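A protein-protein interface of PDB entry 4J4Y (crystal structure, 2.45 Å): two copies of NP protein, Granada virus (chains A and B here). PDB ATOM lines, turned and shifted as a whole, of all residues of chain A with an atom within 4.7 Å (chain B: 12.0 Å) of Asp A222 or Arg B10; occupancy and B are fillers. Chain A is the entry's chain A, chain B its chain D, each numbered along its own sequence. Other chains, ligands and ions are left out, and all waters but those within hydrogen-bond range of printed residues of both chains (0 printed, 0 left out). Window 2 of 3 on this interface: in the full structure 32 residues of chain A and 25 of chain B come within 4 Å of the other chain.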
ATOM      1  N   PHE A 217      32.332   4.331   9.408  1.00  0.00           N
ATOM      2  CA  PHE A 217      31.438   4.790  10.437  1.00  0.00           C
ATOM      3  C   PHE A 217      30.073   5.205   9.934  1.00  0.00           C
ATOM      4  O   PHE A 217      29.079   4.924  10.531  1.00  0.00           O
ATOM      5  CB  PHE A 217      32.118   5.952  11.117  1.00  0.00           C
ATOM      6  CG  PHE A 217      31.339   6.573  12.216  1.00  0.00           C
ATOM      7  CD1 PHE A 217      30.848   5.826  13.233  1.00  0.00           C
ATOM      8  CD2 PHE A 217      31.134   7.926  12.226  1.00  0.00           C
ATOM      9  CE1 PHE A 217      30.143   6.411  14.241  1.00  0.00           C
ATOM     10  CE2 PHE A 217      30.451   8.520  13.228  1.00  0.00           C
ATOM     11  CZ  PHE A 217      29.945   7.758  14.235  1.00  0.00           C
ATOM     12  N   PHE A 218      30.046   5.877   8.814  1.00  0.00           N
ATOM     13  CA  PHE A 218      28.816   6.285   8.225  1.00  0.00           C
ATOM     14  C   PHE A 218      28.659   5.389   7.041  1.00  0.00           C
ATOM     15  O   PHE A 218      29.616   5.041   6.418  1.00  0.00           O
ATOM     16  CB  PHE A 218      28.895   7.728   7.776  1.00  0.00           C
ATOM     17  CG  PHE A 218      28.772   8.727   8.878  1.00  0.00           C
ATOM     18  CD1 PHE A 218      27.802   8.625   9.813  1.00  0.00           C
ATOM     19  CD2 PHE A 218      29.614   9.788   8.941  1.00  0.00           C
ATOM     20  CE1 PHE A 218      27.686   9.553  10.806  1.00  0.00           C
ATOM     21  CE2 PHE A 218      29.508  10.711   9.939  1.00  0.00           C
ATOM     22  CZ  PHE A 218      28.540  10.597  10.869  1.00  0.00           C
ATOM     23  N   THR A 219      27.454   4.960   6.775  1.00  0.00           N
ATOM     24  CA  THR A 219      27.159   4.163   5.616  1.00  0.00           C
ATOM     25  C   THR A 219      26.957   4.982   4.391  1.00  0.00           C
ATOM     26  O   THR A 219      26.806   6.162   4.458  1.00  0.00           O
ATOM     27  CB  THR A 219      25.953   3.251   5.832  1.00  0.00           C
ATOM     28  OG1 THR A 219      24.784   4.025   5.978  1.00  0.00           O
ATOM     29  CG2 THR A 219      26.134   2.461   7.055  1.00  0.00           C
ATOM     30  N   ARG A 220      26.913   4.314   3.265  1.00  0.00           N
ATOM     31  CA  ARG A 220      26.723   4.968   2.003  1.00  0.00           C
ATOM     32  C   ARG A 220      25.397   5.658   1.989  1.00  0.00           C
ATOM     33  O   ARG A 220      25.247   6.702   1.443  1.00  0.00           O
ATOM     34  CB  ARG A 220      26.819   3.974   0.873  1.00  0.00           C
ATOM     35  CG  ARG A 220      28.164   3.976   0.206  1.00  0.00           C
ATOM     36  CD  ARG A 220      28.315   2.870  -0.795  1.00  0.00           C
ATOM     37  NE  ARG A 220      27.450   3.035  -1.939  1.00  0.00           N
ATOM     38  CZ  ARG A 220      27.387   4.126  -2.672  1.00  0.00           C
ATOM     39  NH1 ARG A 220      28.147   5.177  -2.392  1.00  0.00           N
ATOM     40  NH2 ARG A 220      26.555   4.159  -3.678  1.00  0.00           N
ATOM     41  N   ASP A 221      24.434   5.042   2.604  1.00  0.00           N
ATOM     42  CA  ASP A 221      23.156   5.626   2.748  1.00  0.00           C
ATOM     43  C   ASP A 221      23.097   6.859   3.596  1.00  0.00           C
ATOM     44  O   ASP A 221      22.378   7.756   3.278  1.00  0.00           O
ATOM     45  CB  ASP A 221      22.164   4.614   3.232  1.00  0.00           C
ATOM     46  CG  ASP A 221      20.901   4.702   2.498  1.00  0.00           C
ATOM     47  OD1 ASP A 221      20.796   4.071   1.448  1.00  0.00           O
ATOM     48  OD2 ASP A 221      20.022   5.444   2.935  1.00  0.00           O
ATOM     49  N   ASP A 222      23.839   6.877   4.674  1.00  0.00           N
ATOM     50  CA  ASP A 222      23.940   8.046   5.495  1.00  0.00           C
ATOM     51  C   ASP A 222      24.564   9.197   4.780  1.00  0.00           C
ATOM     52  O   ASP A 222      24.125  10.291   4.891  1.00  0.00           O
ATOM     53  CB  ASP A 222      24.779   7.761   6.712  1.00  0.00           C
ATOM     54  CG  ASP A 222      24.217   6.702   7.561  1.00  0.00           C
ATOM     55  OD1 ASP A 222      23.010   6.659   7.748  1.00  0.00           O
ATOM     56  OD2 ASP A 222      24.995   5.914   8.064  1.00  0.00           O
ATOM     57  N   LYS A 223      25.605   8.923   4.038  1.00  0.00           N
ATOM     58  CA  LYS A 223      26.298   9.965   3.344  1.00  0.00           C
ATOM     59  C   LYS A 223      25.389  10.625   2.349  1.00  0.00           C
ATOM     60  O   LYS A 223      25.380  11.817   2.210  1.00  0.00           O
ATOM     61  CB  LYS A 223      27.532   9.412   2.681  1.00  0.00           C
ATOM     62  CG  LYS A 223      28.624   9.166   3.664  1.00  0.00           C
ATOM     63  CD  LYS A 223      29.638   8.248   3.077  1.00  0.00           C
ATOM     64  CE  LYS A 223      30.897   8.301   3.874  1.00  0.00           C
ATOM     65  NZ  LYS A 223      31.940   7.530   3.211  1.00  0.00           N
ATOM     66  N   LYS A 224      24.581   9.820   1.698  1.00  0.00           N
ATOM     67  CA  LYS A 224      23.679  10.320   0.730  1.00  0.00           C
ATOM     68  C   LYS A 224      22.757  11.247   1.421  1.00  0.00           C
ATOM     69  O   LYS A 224      22.436  12.274   0.915  1.00  0.00           O
ATOM     70  CB  LYS A 224      22.854   9.172   0.186  1.00  0.00           C
ATOM     71  CG  LYS A 224      23.521   8.339  -0.878  1.00  0.00           C
ATOM     72  CD  LYS A 224      22.620   7.193  -1.244  1.00  0.00           C
ATOM     73  CE  LYS A 224      23.095   6.426  -2.450  1.00  0.00           C
ATOM     74  NZ  LYS A 224      21.910   5.760  -3.027  1.00  0.00           N
ATOM     75  N   LYS A 225      22.301  10.840   2.580  1.00  0.00           N
ATOM     76  CA  LYS A 225      21.322  11.578   3.301  1.00  0.00           C
ATOM     77  C   LYS A 225      21.833  12.943   3.709  1.00  0.00           C
ATOM     78  O   LYS A 225      21.166  13.903   3.544  1.00  0.00           O
ATOM     79  CB  LYS A 225      20.891  10.756   4.509  1.00  0.00           C
ATOM     80  CG  LYS A 225      19.812  11.374   5.379  1.00  0.00           C
ATOM     81  CD  LYS A 225      20.319  11.779   6.754  1.00  0.00           C
ATOM     82  CE  LYS A 225      19.310  11.483   7.853  1.00  0.00           C
ATOM     83  NZ  LYS A 225      19.894  11.554   9.223  1.00  0.00           N
ATOM     84  N   LEU A 226      23.027  13.001   4.237  1.00  0.00           N
ATOM     85  CA  LEU A 226      23.633  14.251   4.614  1.00  0.00           C
ATOM     86  C   LEU A 226      23.941  15.188   3.494  1.00  0.00           C
ATOM     87  O   LEU A 226      23.688  16.340   3.589  1.00  0.00           O
ATOM     88  CB  LEU A 226      24.904  13.989   5.373  1.00  0.00           C
ATOM     89  CG  LEU A 226      24.717  13.131   6.591  1.00  0.00           C
ATOM     90  CD1 LEU A 226      26.005  12.457   6.952  1.00  0.00           C
ATOM     91  CD2 LEU A 226      24.174  13.941   7.727  1.00  0.00           C
ATOM     92  N   GLU B   6      21.776   6.784  23.486  1.00  0.00           N
ATOM     93  CA  GLU B   6      22.765   6.533  24.531  1.00  0.00           C
ATOM     94  C   GLU B   6      23.847   5.536  24.150  1.00  0.00           C
ATOM     95  O   GLU B   6      24.937   5.614  24.637  1.00  0.00           O
ATOM     96  CB  GLU B   6      22.085   6.063  25.820  1.00  0.00           C
ATOM     97  CG  GLU B   6      20.916   6.903  26.285  1.00  0.00           C
ATOM     98  CD  GLU B   6      21.309   8.041  27.198  1.00  0.00           C
ATOM     99  OE1 GLU B   6      21.093   9.191  26.818  1.00  0.00           O
ATOM    100  OE2 GLU B   6      21.796   7.791  28.308  1.00  0.00           O
ATOM    101  N   ASP B   7      23.508   4.564  23.319  1.00  0.00           N
ATOM    102  CA  ASP B   7      24.452   3.539  22.955  1.00  0.00           C
ATOM    103  C   ASP B   7      24.714   3.257  21.489  1.00  0.00           C
ATOM    104  O   ASP B   7      25.544   2.435  21.197  1.00  0.00           O
ATOM    105  CB  ASP B   7      24.087   2.260  23.672  1.00  0.00           C
ATOM    106  CG  ASP B   7      22.724   1.775  23.324  1.00  0.00           C
ATOM    107  OD1 ASP B   7      22.093   2.345  22.403  1.00  0.00           O
ATOM    108  OD2 ASP B   7      22.296   0.796  23.970  1.00  0.00           O
ATOM    109  N   ASN B   8      24.014   3.898  20.576  1.00  0.00           N
ATOM    110  CA  ASN B   8      24.406   3.806  19.182  1.00  0.00           C
ATOM    111  C   ASN B   8      25.075   5.080  18.731  1.00  0.00           C
ATOM    112  O   ASN B   8      24.458   6.069  18.514  1.00  0.00           O
ATOM    113  CB  ASN B   8      23.218   3.473  18.295  1.00  0.00           C
ATOM    114  CG  ASN B   8      23.617   3.145  16.884  1.00  0.00           C
ATOM    115  OD1 ASN B   8      24.586   3.637  16.396  1.00  0.00           O
ATOM    116  ND2 ASN B   8      22.864   2.313  16.235  1.00  0.00           N
ATOM    117  N   TYR B   9      26.378   5.015  18.659  1.00  0.00           N
ATOM    118  CA  TYR B   9      27.228   6.149  18.398  1.00  0.00           C
ATOM    119  C   TYR B   9      27.061   6.738  17.042  1.00  0.00           C
ATOM    120  O   TYR B   9      27.136   7.912  16.888  1.00  0.00           O
ATOM    121  CB  TYR B   9      28.676   5.804  18.741  1.00  0.00           C
ATOM    122  CG  TYR B   9      28.765   5.337  20.153  1.00  0.00           C
ATOM    123  CD1 TYR B   9      28.321   6.134  21.168  1.00  0.00           C
ATOM    124  CD2 TYR B   9      29.226   4.090  20.474  1.00  0.00           C
ATOM    125  CE1 TYR B   9      28.354   5.723  22.463  1.00  0.00           C
ATOM    126  CE2 TYR B   9      29.257   3.680  21.778  1.00  0.00           C
ATOM    127  CZ  TYR B   9      28.812   4.505  22.762  1.00  0.00           C
ATOM    128  OH  TYR B   9      28.830   4.112  24.059  1.00  0.00           O
ATOM    129  N   ARG B  10      26.868   5.893  16.063  1.00  0.00           N
ATOM    130  CA  ARG B  10      26.681   6.357  14.730  1.00  0.00           C
ATOM    131  C   ARG B  10      25.424   7.159  14.602  1.00  0.00           C
ATOM    132  O   ARG B  10      25.407   8.172  13.976  1.00  0.00           O
ATOM    133  CB  ARG B  10      26.654   5.168  13.812  1.00  0.00           C
ATOM    134  CG  ARG B  10      26.149   5.429  12.431  1.00  0.00           C
ATOM    135  CD  ARG B  10      26.052   4.157  11.619  1.00  0.00           C
ATOM    136  NE  ARG B  10      25.000   4.238  10.636  1.00  0.00           N
ATOM    137  CZ  ARG B  10      23.730   4.048  10.909  1.00  0.00           C
ATOM    138  NH1 ARG B  10      23.349   3.727  12.108  1.00  0.00           N
ATOM    139  NH2 ARG B  10      22.838   4.161   9.978  1.00  0.00           N
ATOM    140  N   THR B  11      24.350   6.652  15.161  1.00  0.00           N
ATOM    141  CA  THR B  11      23.096   7.341  15.194  1.00  0.00           C
ATOM    142  C   THR B  11      23.074   8.579  16.064  1.00  0.00           C
ATOM    143  O   THR B  11      22.421   9.508  15.741  1.00  0.00           O
ATOM    144  CB  THR B  11      21.885   6.403  15.363  1.00  0.00           C
ATOM    145  OG1 THR B  11      21.910   5.772  16.620  1.00  0.00           O
ATOM    146  CG2 THR B  11      21.925   5.373  14.364  1.00  0.00           C
ATOM    147  N   ILE B  12      23.793   8.569  17.168  1.00  0.00           N
ATOM    148  CA  ILE B  12      23.883   9.738  17.982  1.00  0.00           C
ATOM    149  C   ILE B  12      24.521  10.826  17.162  1.00  0.00           C
ATOM    150  O   ILE B  12      24.044  11.914  17.114  1.00  0.00           O
ATOM    151  CB  ILE B  12      24.712   9.480  19.244  1.00  0.00           C
ATOM    152  CG1 ILE B  12      23.946   8.622  20.216  1.00  0.00           C
ATOM    153  CG2 ILE B  12      25.015  10.751  19.972  1.00  0.00           C
ATOM    154  CD1 ILE B  12      24.771   8.070  21.344  1.00  0.00           C
ATOM    155  N   ALA B  13      25.584  10.502  16.465  1.00  0.00           N
ATOM    156  CA  ALA B  13      26.235  11.453  15.608  1.00  0.00           C
ATOM    157  C   ALA B  13      25.393  11.948  14.443  1.00  0.00           C
ATOM    158  O   ALA B  13      25.368  13.111  14.183  1.00  0.00           O
ATOM    159  CB  ALA B  13      27.547  10.898  15.131  1.00  0.00           C
ATOM    160  N   LEU B  14      24.658  11.073  13.795  1.00  0.00           N
ATOM    161  CA  LEU B  14      23.775  11.461  12.740  1.00  0.00           C
ATOM    162  C   LEU B  14      22.686  12.405  13.176  1.00  0.00           C
ATOM    163  O   LEU B  14      22.249  13.205  12.418  1.00  0.00           O
ATOM    164  CB  LEU B  14      23.188  10.257  12.057  1.00  0.00           C
ATOM    165  CG  LEU B  14      24.155   9.560  11.137  1.00  0.00           C
ATOM    166  CD1 LEU B  14      23.642   8.227  10.660  1.00  0.00           C
ATOM    167  CD2 LEU B  14      24.548  10.428   9.975  1.00  0.00           C
ATOM    168  N   ALA B  15      22.289  12.327  14.431  1.00  0.00           N
ATOM    169  CA  ALA B  15      21.227  13.126  14.971  1.00  0.00           C
ATOM    170  C   ALA B  15      21.633  14.554  15.103  1.00  0.00           C
ATOM    171  O   ALA B  15      20.815  15.398  15.294  1.00  0.00           O
ATOM    172  CB  ALA B  15      20.768  12.586  16.293  1.00  0.00           C
ATOM    173  N   PHE B  16      22.906  14.814  14.973  1.00  0.00           N
ATOM    174  CA  PHE B  16      23.388  16.161  15.035  1.00  0.00           C
ATOM    175  C   PHE B  16      23.007  16.982  13.823  1.00  0.00           C
ATOM    176  O   PHE B  16      23.066  18.173  13.858  1.00  0.00           O
ATOM    177  CB  PHE B  16      24.872  16.216  15.315  1.00  0.00           C
ATOM    178  CG  PHE B  16      25.201  16.326  16.759  1.00  0.00           C
ATOM    179  CD1 PHE B  16      25.014  15.271  17.614  1.00  0.00           C
ATOM    180  CD2 PHE B  16      25.688  17.472  17.264  1.00  0.00           C
ATOM    181  CE1 PHE B  16      25.317  15.371  18.939  1.00  0.00           C
ATOM    182  CE2 PHE B  16      25.992  17.577  18.584  1.00  0.00           C
ATOM    183  CZ  PHE B  16      25.813  16.530  19.422  1.00  0.00           C
ATOM    184  N   LEU B  17      22.551  16.333  12.776  1.00  0.00           N
ATOM    185  CA  LEU B  17      22.096  17.026  11.607  1.00  0.00           C
ATOM    186  C   LEU B  17      20.938  17.913  11.993  1.00  0.00           C
ATOM    187  O   LEU B  17      20.744  18.965  11.453  1.00  0.00           O
ATOM    188  CB  LEU B  17      21.688  16.049  10.529  1.00  0.00           C
ATOM    189  CG  LEU B  17      21.105  16.635   9.255  1.00  0.00           C
ATOM    190  CD1 LEU B  17      22.136  17.412   8.489  1.00  0.00           C
ATOM    191  CD2 LEU B  17      20.461  15.608   8.383  1.00  0.00           C
ATOM    192  N   ASP B  18      20.169  17.462  12.958  1.00  0.00           N
ATOM    193  CA  ASP B  18      19.001  18.169  13.397  1.00  0.00           C
ATOM    194  C   ASP B  18      19.168  18.944  14.674  1.00  0.00           C
ATOM    195  O   ASP B  18      18.248  19.520  15.148  1.00  0.00           O
ATOM    196  CB  ASP B  18      17.842  17.206  13.498  1.00  0.00           C
ATOM    197  CG  ASP B  18      17.539  16.550  12.207  1.00  0.00           C
ATOM    198  OD1 ASP B  18      17.479  17.225  11.208  1.00  0.00           O
ATOM    199  OD2 ASP B  18      17.345  15.358  12.169  1.00  0.00           O
ATOM    200  N   GLU B  19      20.354  18.948  15.230  1.00  0.00           N
ATOM    201  CA  GLU B  19      20.638  19.758  16.378  1.00  0.00           C
ATOM    202  C   GLU B  19      20.651  21.191  15.935  1.00  0.00           C
ATOM    203  O   GLU B  19      20.963  21.489  14.823  1.00  0.00           O
ATOM    204  CB  GLU B  19      21.971  19.378  16.981  1.00  0.00           C
ATOM    205  CG  GLU B  19      21.909  18.190  17.894  1.00  0.00           C
ATOM    206  CD  GLU B  19      21.233  18.500  19.203  1.00  0.00           C
ATOM    207  OE1 GLU B  19      21.060  19.665  19.509  1.00  0.00           O
ATOM    208  OE2 GLU B  19      20.853  17.582  19.910  1.00  0.00           O
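O of Tyr B9 touches CZ of Phe A217 (3.9 Å). Arg B10 touches Phe A217. CD2 of Leu B14 touches CE1 of Phe A218 (3.4 Å). OD1 of Asp A222 touches CD1 of Leu B14 (3.4 Å). Leu A226 touches Leu B14 (CD1 to CD2, 3.9 Å).
Of the 10 printed residues of chain A, 4 touch a printed residue of chain B. Of the 14 printed residues of chain B, 3 touch a printed residue of chain A. Hydrophobic or aromatic side chains of chain B that line the printed part of chain A: Leu B14. Among the printed residues, Asp or Glu carboxylates within 4 Å of a Lys or Arg side-chain nitrogen of the other chain: Asp A222 with Arg B10.
No position is printed for both chains. Of the 6 pairs that touch across the chains among the printed residues, none has its exchanged pair printed and touching as well.
Of chain B, only Arg B10 (3.1 Å) and Leu B14 (3.4 Å) come within 4 Å of Asp A222. Of the printed residues of chain A, Arg B10 touches Phe A217 (3.3 Å) and Asp A222 (3.1 Å). Printed residues of chain B within 4 Å of Phe A217: Tyr B9 (3.9 Å) and Arg B10 (3.3 Å). Of the printed residues of chain B, Phe A218 touches Leu B14. No residue of chain B comes within 4 Å of Thr A219. No residue of chain B comes within 4 Å of Lys A223. No residue of chain B comes within 4 Å of Lys A225. Printed residues of chain A within 4 Å of Leu B14: Phe A218, Asp A222 and Leu A226. Of the printed residues of chain A, Tyr B9 touches Phe A217 (3.9 Å). Ala B13 touches none of the printed residues of chain A. Glu B19 touches none of the printed residues of chain A. The nearest residue of chain B that does not touch Asp A222 is Thr B11 (6.8 Å). The nearest printed residue of chain A that does not touch Arg B10 is Phe A218 (4.1 Å).
OD2 of Asp A222 is in salt-bridge range of NE of Arg B10, at 3.1 Å.
The side-chain amide oxygen (OD1) of Asn B8 lies within hydrogen-bond range of the backbone NH (N) of Arg B10. The side-chain hydroxyl of Thr A219 lies within hydrogen-bond range of the side-chain carboxylate of Asp A222 (2.8 Å).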
